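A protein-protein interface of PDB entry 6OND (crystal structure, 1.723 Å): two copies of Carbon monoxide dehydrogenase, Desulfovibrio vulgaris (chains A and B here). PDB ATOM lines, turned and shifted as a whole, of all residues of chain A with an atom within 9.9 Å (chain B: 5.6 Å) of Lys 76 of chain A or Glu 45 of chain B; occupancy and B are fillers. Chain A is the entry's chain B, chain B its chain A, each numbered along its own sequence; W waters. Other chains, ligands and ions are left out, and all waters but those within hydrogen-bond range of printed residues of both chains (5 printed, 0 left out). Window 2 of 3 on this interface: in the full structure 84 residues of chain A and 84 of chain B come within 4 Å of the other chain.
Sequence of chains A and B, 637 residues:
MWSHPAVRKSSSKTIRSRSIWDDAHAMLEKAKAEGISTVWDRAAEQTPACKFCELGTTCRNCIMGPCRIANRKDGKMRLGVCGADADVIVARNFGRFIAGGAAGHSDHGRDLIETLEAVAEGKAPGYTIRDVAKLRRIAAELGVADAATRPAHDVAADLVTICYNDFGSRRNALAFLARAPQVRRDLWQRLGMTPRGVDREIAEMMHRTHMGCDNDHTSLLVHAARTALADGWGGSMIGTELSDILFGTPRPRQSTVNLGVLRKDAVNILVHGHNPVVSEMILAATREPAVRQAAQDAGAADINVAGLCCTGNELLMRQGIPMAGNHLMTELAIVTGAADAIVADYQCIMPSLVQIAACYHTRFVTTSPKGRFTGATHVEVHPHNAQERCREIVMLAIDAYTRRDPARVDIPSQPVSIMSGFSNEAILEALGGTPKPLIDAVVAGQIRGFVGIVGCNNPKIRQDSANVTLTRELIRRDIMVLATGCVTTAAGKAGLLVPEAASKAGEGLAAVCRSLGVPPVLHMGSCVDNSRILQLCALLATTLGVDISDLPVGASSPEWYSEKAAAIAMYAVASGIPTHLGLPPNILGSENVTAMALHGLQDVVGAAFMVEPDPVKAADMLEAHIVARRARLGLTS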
ATOM      1  N   PHE A  52      12.245 -13.284   9.248  1.00  0.00           N
ATOM      2  CA  PHE A  52      11.864 -13.496   7.853  1.00  0.00           C
ATOM      3  C   PHE A  52      10.689 -12.613   7.462  1.00  0.00           C
ATOM      4  O   PHE A  52      10.677 -12.049   6.364  1.00  0.00           O
ATOM      5  CB  PHE A  52      11.499 -14.968   7.607  1.00  0.00           C
ATOM      6  CG  PHE A  52      12.619 -15.928   7.889  1.00  0.00           C
ATOM      7  CD1 PHE A  52      13.563 -16.217   6.912  1.00  0.00           C
ATOM      8  CD2 PHE A  52      12.723 -16.547   9.123  1.00  0.00           C
ATOM      9  CE1 PHE A  52      14.596 -17.106   7.163  1.00  0.00           C
ATOM     10  CE2 PHE A  52      13.754 -17.438   9.377  1.00  0.00           C
ATOM     11  CZ  PHE A  52      14.690 -17.710   8.393  1.00  0.00           C
ATOM     12  N   MET A  64       2.123 -25.996  -0.854  1.00  0.00           N
ATOM     13  CA  MET A  64       3.437 -26.622  -0.960  1.00  0.00           C
ATOM     14  C   MET A  64       4.379 -26.042   0.087  1.00  0.00           C
ATOM     15  O   MET A  64       5.262 -26.745   0.589  1.00  0.00           O
ATOM     16  CB  MET A  64       4.029 -26.479  -2.368  1.00  0.00           C
ATOM     17  CG  MET A  64       3.212 -27.159  -3.485  1.00  0.00           C
ATOM     18  SD  MET A  64       4.276 -27.594  -4.896  1.00  0.00           S
ATOM     19  CE  MET A  64       4.890 -25.980  -5.350  1.00  0.00           C
ATOM     20  N   GLY A  65       4.188 -24.769   0.430  1.00  0.00           N
ATOM     21  CA  GLY A  65       4.877 -24.141   1.529  1.00  0.00           C
ATOM     22  C   GLY A  65       4.119 -24.373   2.822  1.00  0.00           C
ATOM     23  O   GLY A  65       3.369 -25.347   2.951  1.00  0.00           O
ATOM     24  N   PRO A  66       4.266 -23.469   3.801  1.00  0.00           N
ATOM     25  CA  PRO A  66       4.947 -22.172   3.690  1.00  0.00           C
ATOM     26  C   PRO A  66       6.466 -22.290   3.555  1.00  0.00           C
ATOM     27  O   PRO A  66       7.060 -23.314   3.940  1.00  0.00           O
ATOM     28  CB  PRO A  66       4.565 -21.470   4.996  1.00  0.00           C
ATOM     29  CG  PRO A  66       4.368 -22.600   5.974  1.00  0.00           C
ATOM     30  CD  PRO A  66       3.744 -23.712   5.158  1.00  0.00           C
ATOM     31  N   CYS A  67       7.083 -21.249   3.012  1.00  0.00           N
ATOM     32  CA  CYS A  67       8.503 -21.268   2.695  1.00  0.00           C
ATOM     33  C   CYS A  67       9.191 -20.077   3.334  1.00  0.00           C
ATOM     34  O   CYS A  67       8.599 -19.004   3.481  1.00  0.00           O
ATOM     35  CB  CYS A  67       8.732 -21.185   1.175  1.00  0.00           C
ATOM     36  SG  CYS A  67       7.969 -22.551   0.251  1.00  0.00           S
ATOM     37  N   ARG A  68      10.461 -20.273   3.686  1.00  0.00           N
ATOM     38  CA  ARG A  68      11.325 -19.201   4.162  1.00  0.00           C
ATOM     39  C   ARG A  68      12.612 -19.218   3.344  1.00  0.00           C
ATOM     40  O   ARG A  68      13.112 -20.284   2.977  1.00  0.00           O
ATOM     41  CB  ARG A  68      11.683 -19.397   5.639  1.00  0.00           C
ATOM     42  CG  ARG A  68      10.592 -18.967   6.623  1.00  0.00           C
ATOM     43  CD  ARG A  68      10.843 -19.554   8.003  1.00  0.00           C
ATOM     44  NE  ARG A  68      10.830 -21.015   7.930  1.00  0.00           N
ATOM     45  CZ  ARG A  68      11.193 -21.830   8.913  1.00  0.00           C
ATOM     46  NH1 ARG A  68      11.590 -21.338  10.077  1.00  0.00           N
ATOM     47  NH2 ARG A  68      11.147 -23.145   8.730  1.00  0.00           N
ATOM     48  N   ILE A  69      13.175 -18.036   3.096  1.00  0.00           N
ATOM     49  CA  ILE A  69      14.404 -17.909   2.314  1.00  0.00           C
ATOM     50  C   ILE A  69      15.526 -17.468   3.237  1.00  0.00           C
ATOM     51  O   ILE A  69      15.424 -16.424   3.896  1.00  0.00           O
ATOM     52  CB  ILE A  69      14.255 -16.911   1.162  1.00  0.00           C
ATOM     53  CG1 ILE A  69      13.111 -17.328   0.244  1.00  0.00           C
ATOM     54  CG2 ILE A  69      15.559 -16.830   0.365  1.00  0.00           C
ATOM     55  CD1 ILE A  69      13.254 -18.746  -0.322  1.00  0.00           C
ATOM     56  N   ALA A  70      16.594 -18.252   3.279  1.00  0.00           N
ATOM     57  CA  ALA A  70      17.820 -17.857   3.953  1.00  0.00           C
ATOM     58  C   ALA A  70      18.902 -17.541   2.926  1.00  0.00           C
ATOM     59  O   ALA A  70      18.790 -17.878   1.740  1.00  0.00           O
ATOM     60  CB  ALA A  70      18.302 -18.964   4.895  1.00  0.00           C
ATOM     61  N   ASN A  71      19.956 -16.877   3.395  1.00  0.00           N
ATOM     62  CA  ASN A  71      21.153 -16.604   2.597  1.00  0.00           C
ATOM     63  C   ASN A  71      22.308 -17.341   3.269  1.00  0.00           C
ATOM     64  O   ASN A  71      22.933 -16.824   4.196  1.00  0.00           O
ATOM     65  CB  ASN A  71      21.419 -15.102   2.496  1.00  0.00           C
ATOM     66  N   ARG A  72      22.578 -18.559   2.805  1.00  0.00           N
ATOM     67  CA  ARG A  72      23.624 -19.407   3.358  1.00  0.00           C
ATOM     68  C   ARG A  72      24.625 -19.774   2.270  1.00  0.00           C
ATOM     69  O   ARG A  72      24.285 -19.842   1.085  1.00  0.00           O
ATOM     70  CB  ARG A  72      23.040 -20.693   3.962  1.00  0.00           C
ATOM     71  CG  ARG A  72      22.067 -20.455   5.100  1.00  0.00           C
ATOM     72  CD  ARG A  72      21.511 -21.763   5.651  1.00  0.00           C
ATOM     73  NE  ARG A  72      20.408 -21.529   6.584  1.00  0.00           N
ATOM     74  CZ  ARG A  72      19.698 -22.489   7.175  1.00  0.00           C
ATOM     75  NH1 ARG A  72      19.970 -23.766   6.941  1.00  0.00           N
ATOM     76  NH2 ARG A  72      18.712 -22.171   8.005  1.00  0.00           N
ATOM     77  N   LYS A  73      25.870 -20.017   2.691  1.00  0.00           N
ATOM     78  CA  LYS A  73      26.917 -20.367   1.734  1.00  0.00           C
ATOM     79  C   LYS A  73      26.631 -21.707   1.069  1.00  0.00           C
ATOM     80  O   LYS A  73      26.891 -21.883  -0.129  1.00  0.00           O
ATOM     81  CB  LYS A  73      28.280 -20.383   2.427  1.00  0.00           C
ATOM     82  N   ASP A  74      26.097 -22.667   1.827  1.00  0.00           N
ATOM     83  CA  ASP A  74      25.768 -23.965   1.247  1.00  0.00           C
ATOM     84  C   ASP A  74      24.551 -23.918   0.332  1.00  0.00           C
ATOM     85  O   ASP A  74      24.280 -24.906  -0.360  1.00  0.00           O
ATOM     86  CB  ASP A  74      25.615 -25.041   2.334  1.00  0.00           C
ATOM     87  CG  ASP A  74      24.575 -24.686   3.384  1.00  0.00           C
ATOM     88  OD1 ASP A  74      23.650 -23.896   3.092  1.00  0.00           O
ATOM     89  OD2 ASP A  74      24.691 -25.203   4.516  1.00  0.00           O
ATOM     90  N   GLY A  75      23.818 -22.808   0.315  1.00  0.00           N
ATOM     91  CA  GLY A  75      22.716 -22.644  -0.606  1.00  0.00           C
ATOM     92  C   GLY A  75      21.438 -23.367  -0.245  1.00  0.00           C
ATOM     93  O   GLY A  75      20.555 -23.483  -1.103  1.00  0.00           O
ATOM     94  N   LYS A  76      21.309 -23.868   0.983  1.00  0.00           N
ATOM     95  CA  LYS A  76      20.065 -24.487   1.420  1.00  0.00           C
ATOM     96  C   LYS A  76      19.023 -23.418   1.728  1.00  0.00           C
ATOM     97  O   LYS A  76      19.355 -22.293   2.120  1.00  0.00           O
ATOM     98  CB  LYS A  76      20.297 -25.342   2.667  1.00  0.00           C
ATOM     99  N   MET A  77      17.749 -23.782   1.537  1.00  0.00           N
ATOM    100  CA  MET A  77      16.621 -22.854   1.703  1.00  0.00           C
ATOM    101  C   MET A  77      16.840 -21.552   0.945  1.00  0.00           C
ATOM    102  O   MET A  77      16.392 -20.481   1.366  1.00  0.00           O
ATOM    103  CB  MET A  77      16.290 -22.598   3.172  1.00  0.00           C
ATOM    104  CG  MET A  77      15.811 -23.841   3.896  1.00  0.00           C
ATOM    105  SD  MET A  77      15.566 -23.539   5.650  1.00  0.00           S
ATOM    106  CE  MET A  77      14.073 -22.544   5.631  1.00  0.00           C
ATOM    107  N   ARG A  78      17.556 -21.639  -0.174  1.00  0.00           N
ATOM    108  CA  ARG A  78      17.704 -20.501  -1.061  1.00  0.00           C
ATOM    109  C   ARG A  78      16.446 -20.254  -1.877  1.00  0.00           C
ATOM    110  O   ARG A  78      16.207 -19.116  -2.296  1.00  0.00           O
ATOM    111  CB  ARG A  78      18.915 -20.711  -1.986  1.00  0.00           C
ATOM    112  CG  ARG A  78      19.211 -19.532  -2.907  1.00  0.00           C
ATOM    113  CD  ARG A  78      20.449 -19.763  -3.767  1.00  0.00           C
ATOM    114  NE  ARG A  78      20.211 -20.760  -4.807  1.00  0.00           N
ATOM    115  CZ  ARG A  78      19.729 -20.481  -6.014  1.00  0.00           C
ATOM    116  NH1 ARG A  78      19.541 -21.454  -6.893  1.00  0.00           N
ATOM    117  NH2 ARG A  78      19.433 -19.230  -6.345  1.00  0.00           N
ATOM    118  N   LEU A  79      15.616 -21.287  -2.080  1.00  0.00           N
ATOM    119  CA  LEU A  79      14.452 -21.195  -2.945  1.00  0.00           C
ATOM    120  C   LEU A  79      13.233 -21.769  -2.237  1.00  0.00           C
ATOM    121  O   LEU A  79      13.348 -22.654  -1.387  1.00  0.00           O
ATOM    122  CB  LEU A  79      14.660 -22.016  -4.235  1.00  0.00           C
ATOM    123  CG  LEU A  79      15.901 -21.685  -5.077  1.00  0.00           C
ATOM    124  CD1 LEU A  79      16.058 -22.634  -6.265  1.00  0.00           C
ATOM    125  CD2 LEU A  79      15.827 -20.239  -5.539  1.00  0.00           C
ATOM    126  N   GLY A  80      12.062 -21.266  -2.602  1.00  0.00           N
ATOM    127  CA  GLY A  80      10.828 -21.880  -2.155  1.00  0.00           C
ATOM    128  C   GLY A  80      10.601 -23.228  -2.816  1.00  0.00           C
ATOM    129  O   GLY A  80      11.343 -23.661  -3.702  1.00  0.00           O
ATOM    130  N   VAL A  81       9.542 -23.921  -2.379  1.00  0.00           N
ATOM    131  CA  VAL A  81       9.305 -25.265  -2.921  1.00  0.00           C
ATOM    132  C   VAL A  81       9.051 -25.205  -4.424  1.00  0.00           C
ATOM    133  O   VAL A  81       9.502 -26.075  -5.181  1.00  0.00           O
ATOM    134  CB  VAL A  81       8.185 -25.984  -2.143  1.00  0.00           C
ATOM    135  CG1 VAL A  81       7.875 -27.356  -2.768  1.00  0.00           C
ATOM    136  CG2 VAL A  81       8.589 -26.129  -0.685  1.00  0.00           C
ATOM    137  N   GLY A  83      10.448 -23.144  -6.411  1.00  0.00           N
ATOM    138  CA  GLY A  83      11.638 -22.629  -7.061  1.00  0.00           C
ATOM    139  C   GLY A  83      11.801 -21.122  -6.987  1.00  0.00           C
ATOM    140  O   GLY A  83      12.816 -20.606  -7.475  1.00  0.00           O
ATOM    141  N   ALA A  84      10.835 -20.409  -6.404  1.00  0.00           N
ATOM    142  CA  ALA A  84      10.887 -18.951  -6.356  1.00  0.00           C
ATOM    143  C   ALA A  84      12.014 -18.504  -5.435  1.00  0.00           C
ATOM    144  O   ALA A  84      12.230 -19.087  -4.368  1.00  0.00           O
ATOM    145  CB  ALA A  84       9.565 -18.403  -5.809  1.00  0.00           C
ATOM    146  N   TRP B  40      10.583 -32.068  -4.987  1.00  0.00           N
ATOM    147  CA  TRP B  40      10.642 -32.859  -3.758  1.00  0.00           C
ATOM    148  C   TRP B  40      11.880 -32.528  -2.922  1.00  0.00           C
ATOM    149  O   TRP B  40      11.833 -32.591  -1.687  1.00  0.00           O
ATOM    150  CB  TRP B  40      10.610 -34.353  -4.082  1.00  0.00           C
ATOM    151  CG  TRP B  40       9.301 -34.886  -4.638  1.00  0.00           C
ATOM    152  CD1 TRP B  40       8.226 -35.352  -3.921  1.00  0.00           C
ATOM    153  CD2 TRP B  40       8.959 -35.048  -6.020  1.00  0.00           C
ATOM    154  NE1 TRP B  40       7.239 -35.784  -4.781  1.00  0.00           N
ATOM    155  CE2 TRP B  40       7.665 -35.606  -6.071  1.00  0.00           C
ATOM    156  CE3 TRP B  40       9.627 -34.775  -7.222  1.00  0.00           C
ATOM    157  CZ2 TRP B  40       7.022 -35.895  -7.276  1.00  0.00           C
ATOM    158  CZ3 TRP B  40       8.980 -35.055  -8.420  1.00  0.00           C
ATOM    159  CH2 TRP B  40       7.698 -35.614  -8.437  1.00  0.00           C
ATOM    160  N   ASP B  41      13.004 -32.200  -3.569  1.00  0.00           N
ATOM    161  CA  ASP B  41      14.200 -31.833  -2.818  1.00  0.00           C
ATOM    162  C   ASP B  41      14.015 -30.497  -2.119  1.00  0.00           C
ATOM    163  O   ASP B  41      14.474 -30.314  -0.985  1.00  0.00           O
ATOM    164  CB  ASP B  41      15.414 -31.762  -3.745  1.00  0.00           C
ATOM    165  CG  ASP B  41      15.715 -33.084  -4.417  1.00  0.00           C
ATOM    166  OD1 ASP B  41      15.740 -34.122  -3.716  1.00  0.00           O
ATOM    167  OD2 ASP B  41      15.923 -33.084  -5.650  1.00  0.00           O
ATOM    168  N   ARG B  42      13.360 -29.544  -2.787  1.00  0.00           N
ATOM    169  CA  ARG B  42      13.111 -28.248  -2.165  1.00  0.00           C
ATOM    170  C   ARG B  42      12.072 -28.358  -1.055  1.00  0.00           C
ATOM    171  O   ARG B  42      12.181 -27.678  -0.030  1.00  0.00           O
ATOM    172  CB  ARG B  42      12.708 -27.222  -3.228  1.00  0.00           C
ATOM    173  CG  ARG B  42      13.800 -27.028  -4.318  1.00  0.00           C
ATOM    174  CD  ARG B  42      13.469 -25.883  -5.284  1.00  0.00           C
ATOM    175  NE  ARG B  42      12.225 -26.132  -6.010  1.00  0.00           N
ATOM    176  CZ  ARG B  42      12.133 -26.800  -7.160  1.00  0.00           C
ATOM    177  NH1 ARG B  42      13.221 -27.282  -7.756  1.00  0.00           N
ATOM    178  NH2 ARG B  42      10.942 -26.964  -7.727  1.00  0.00           N
ATOM    179  N   ALA B  43      11.068 -29.228  -1.228  1.00  0.00           N
ATOM    180  CA  ALA B  43      10.112 -29.461  -0.152  1.00  0.00           C
ATOM    181  C   ALA B  43      10.816 -29.990   1.089  1.00  0.00           C
ATOM    182  O   ALA B  43      10.510 -29.570   2.213  1.00  0.00           O
ATOM    183  CB  ALA B  43       9.016 -30.429  -0.614  1.00  0.00           C
ATOM    184  N   ALA B  44      11.776 -30.904   0.906  1.00  0.00           N
ATOM    185  CA  ALA B  44      12.517 -31.420   2.050  1.00  0.00           C
ATOM    186  C   ALA B  44      13.328 -30.317   2.718  1.00  0.00           C
ATOM    187  O   ALA B  44      13.470 -30.299   3.947  1.00  0.00           O
ATOM    188  CB  ALA B  44      13.415 -32.581   1.617  1.00  0.00           C
ATOM    189  N   GLU B  45      13.862 -29.378   1.928  1.00  0.00           N
ATOM    190  CA  GLU B  45      14.613 -28.269   2.519  1.00  0.00           C
ATOM    191  C   GLU B  45      13.711 -27.344   3.331  1.00  0.00           C
ATOM    192  O   GLU B  45      14.182 -26.686   4.265  1.00  0.00           O
ATOM    193  CB  GLU B  45      15.343 -27.477   1.435  1.00  0.00           C
ATOM    194  CG  GLU B  45      16.491 -28.231   0.763  1.00  0.00           C
ATOM    195  CD  GLU B  45      17.285 -27.346  -0.190  1.00  0.00           C
ATOM    196  OE1 GLU B  45      17.176 -26.108  -0.079  1.00  0.00           O
ATOM    197  OE2 GLU B  45      18.010 -27.885  -1.054  1.00  0.00           O
ATOM    198  N   GLN B  46      12.425 -27.274   2.997  1.00  0.00           N
ATOM    199  CA  GLN B  46      11.492 -26.380   3.680  1.00  0.00           C
ATOM    200  C   GLN B  46      10.725 -27.062   4.809  1.00  0.00           C
ATOM    201  O   GLN B  46       9.762 -26.485   5.333  1.00  0.00           O
ATOM    202  CB  GLN B  46      10.526 -25.746   2.678  1.00  0.00           C
ATOM    203  CG  GLN B  46      11.210 -24.833   1.660  1.00  0.00           C
ATOM    204  CD  GLN B  46      11.675 -23.519   2.271  1.00  0.00           C
ATOM    205  OE1 GLN B  46      11.243 -23.133   3.365  1.00  0.00           O
ATOM    206  NE2 GLN B  46      12.553 -22.821   1.565  1.00  0.00           N
ATOM    207  N   THR B  47      11.131 -28.271   5.190  1.00  0.00           N
ATOM    208  CA  THR B  47      10.559 -29.014   6.302  1.00  0.00           C
ATOM    209  C   THR B  47      11.603 -29.116   7.399  1.00  0.00           C
ATOM    210  O   THR B  47      12.732 -29.546   7.123  1.00  0.00           O
ATOM    211  CB  THR B  47      10.179 -30.423   5.834  1.00  0.00           C
ATOM    212  OG1 THR B  47       9.281 -30.331   4.721  1.00  0.00           O
ATOM    213  CG2 THR B  47       9.508 -31.201   6.961  1.00  0.00           C
HETATM  214  O   HOH W   1      10.263 -23.731   5.879  1.00  0.00           O
HETATM  215  O   HOH W   2      14.872 -24.743  -0.343  1.00  0.00           O
HETATM  216  O   HOH W   3       7.737 -28.256   2.549  1.00  0.00           O
HETATM  217  O   HOH W   4      13.297 -25.871   7.297  1.00  0.00           O
HETATM  218  O   HOH W   5       7.169 -26.044   4.071  1.00  0.00           O
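O of Gly 80 of chain A lies close to NE of Arg 42 of chain B, 3.5 Å away.
The backbone carbonyl oxygen (O) of Val 81 of chain A is in hydrogen-bond range of the guanidinium group (NE) of Arg 42 of chain B.
The side-chain carboxylate of Glu 45 of chain B is in hydrogen-bond range of the backbone NH of Met 77 of chain A, at 2.9 Å.
NE2 of Gln 46 of chain B lies within hydrogen-bond range of O of Arg 68 of chain A.
NE2 of Gln 46 of chain B lies within hydrogen-bond range of O of Leu 79 of chain A.
N of Gly 83 of chain A lies close to NE of Arg 42 of chain B.
The side-chain hydroxyl (OG1) of Thr 47 of chain B sits at hydrogen-bond distance from the backbone carbonyl oxygen (O) of Ala 43 of chain B.
The backbone NH (N) of Val 81 of chain A sits close to the side-chain sulfur (SG) of Cys 67 of chain A, at 3.4 Å.
N of Ala 70 of chain A sits at hydrogen-bond distance from O of Met 77 of chain A.
N of Lys 76 of chain A sits at hydrogen-bond distance from OD1 of Asp 74 of chain A.
Among the printed residues, pairs that only touch across the chains: Cys 67 of chain A with Gln 46 of chain B (3.4 Å), Lys 76 of chain A with Glu 45 of chain B (3.6 Å), Met 77 of chain A with Gln 46 of chain B (3.7 Å), Val 81 of chain A with Ala 43 of chain B (3.7 Å) and Val 81 of chain A with Gln 46 of chain B (3.7 Å).
Lys 76 of chain A touches one residue of chain B.
Of chain A, only Val 81 (3.7 Å) comes within 4 Å of Ala 43 of chain B.
No residue of chain A comes within 4 Å of Ala 44 of chain B.
Gln 46 of chain B touches just these residues of chain A: Cys 67 (3.4 Å), Arg 68 (3.0 Å), Met 77 (3.7 Å), Leu 79 (3.1 Å) and Val 81 (3.7 Å).
Printed residues of chain B within 4 Å of Met 77 of chain A: Glu 45 and Gln 46.
Of the printed residues of chain B, Gly 80 of chain A touches Arg 42 (3.5 Å).
Printed residues of chain B within 4 Å of Gly 83 of chain A: Arg 42 (3.5 Å).
Asp 74 of chain A touches none of the printed residues of chain B.
The nearest printed residue of chain B that does not touch Gly 83 of chain A is Ala 43 of chain B (8.0 Å).
Printed residues of chain B that touch a printed residue of chain A: Arg 42, Ala 43, Glu 45 and Gln 46.
Hydrophobic or aromatic side chains of chain B that line the printed part of chain A: Ala 43.
Of the 21 printed residues of chain A, 8 touch a printed residue of chain B.
Printed residues of chain A that touch a printed residue of chain B: Cys 67, Arg 68, Lys 76, Met 77, Leu 79, Gly 80, Val 81 and Gly 83.
Hydrophobic or aromatic side chains of chain A that line the printed part of chain B: Met 77 and Val 81.
Among the printed residues, no Asp or Glu carboxylate lies within 4 Å of a Lys or Arg side-chain nitrogen of the other chain.
No position is printed for both chains.
Water W2 lies within hydrogen-bond range of OE1 of Glu 45 of chain B (2.7 Å) and O of Leu 79 of chain A (2.8 Å).
Water W5 lies within hydrogen-bond range of O of Pro 66 of chain A and O of Gln 46 of chain B.
Water W1 bridges OE1 of Gln 46 of chain B (2.8 Å) and NH2 of Arg 68 of chain A (3.0 Å).
Water W4 lies within hydrogen-bond range of O of Glu 45 of chain B (3.3 Å) and SD of Met 77 of chain A (3.6 Å).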
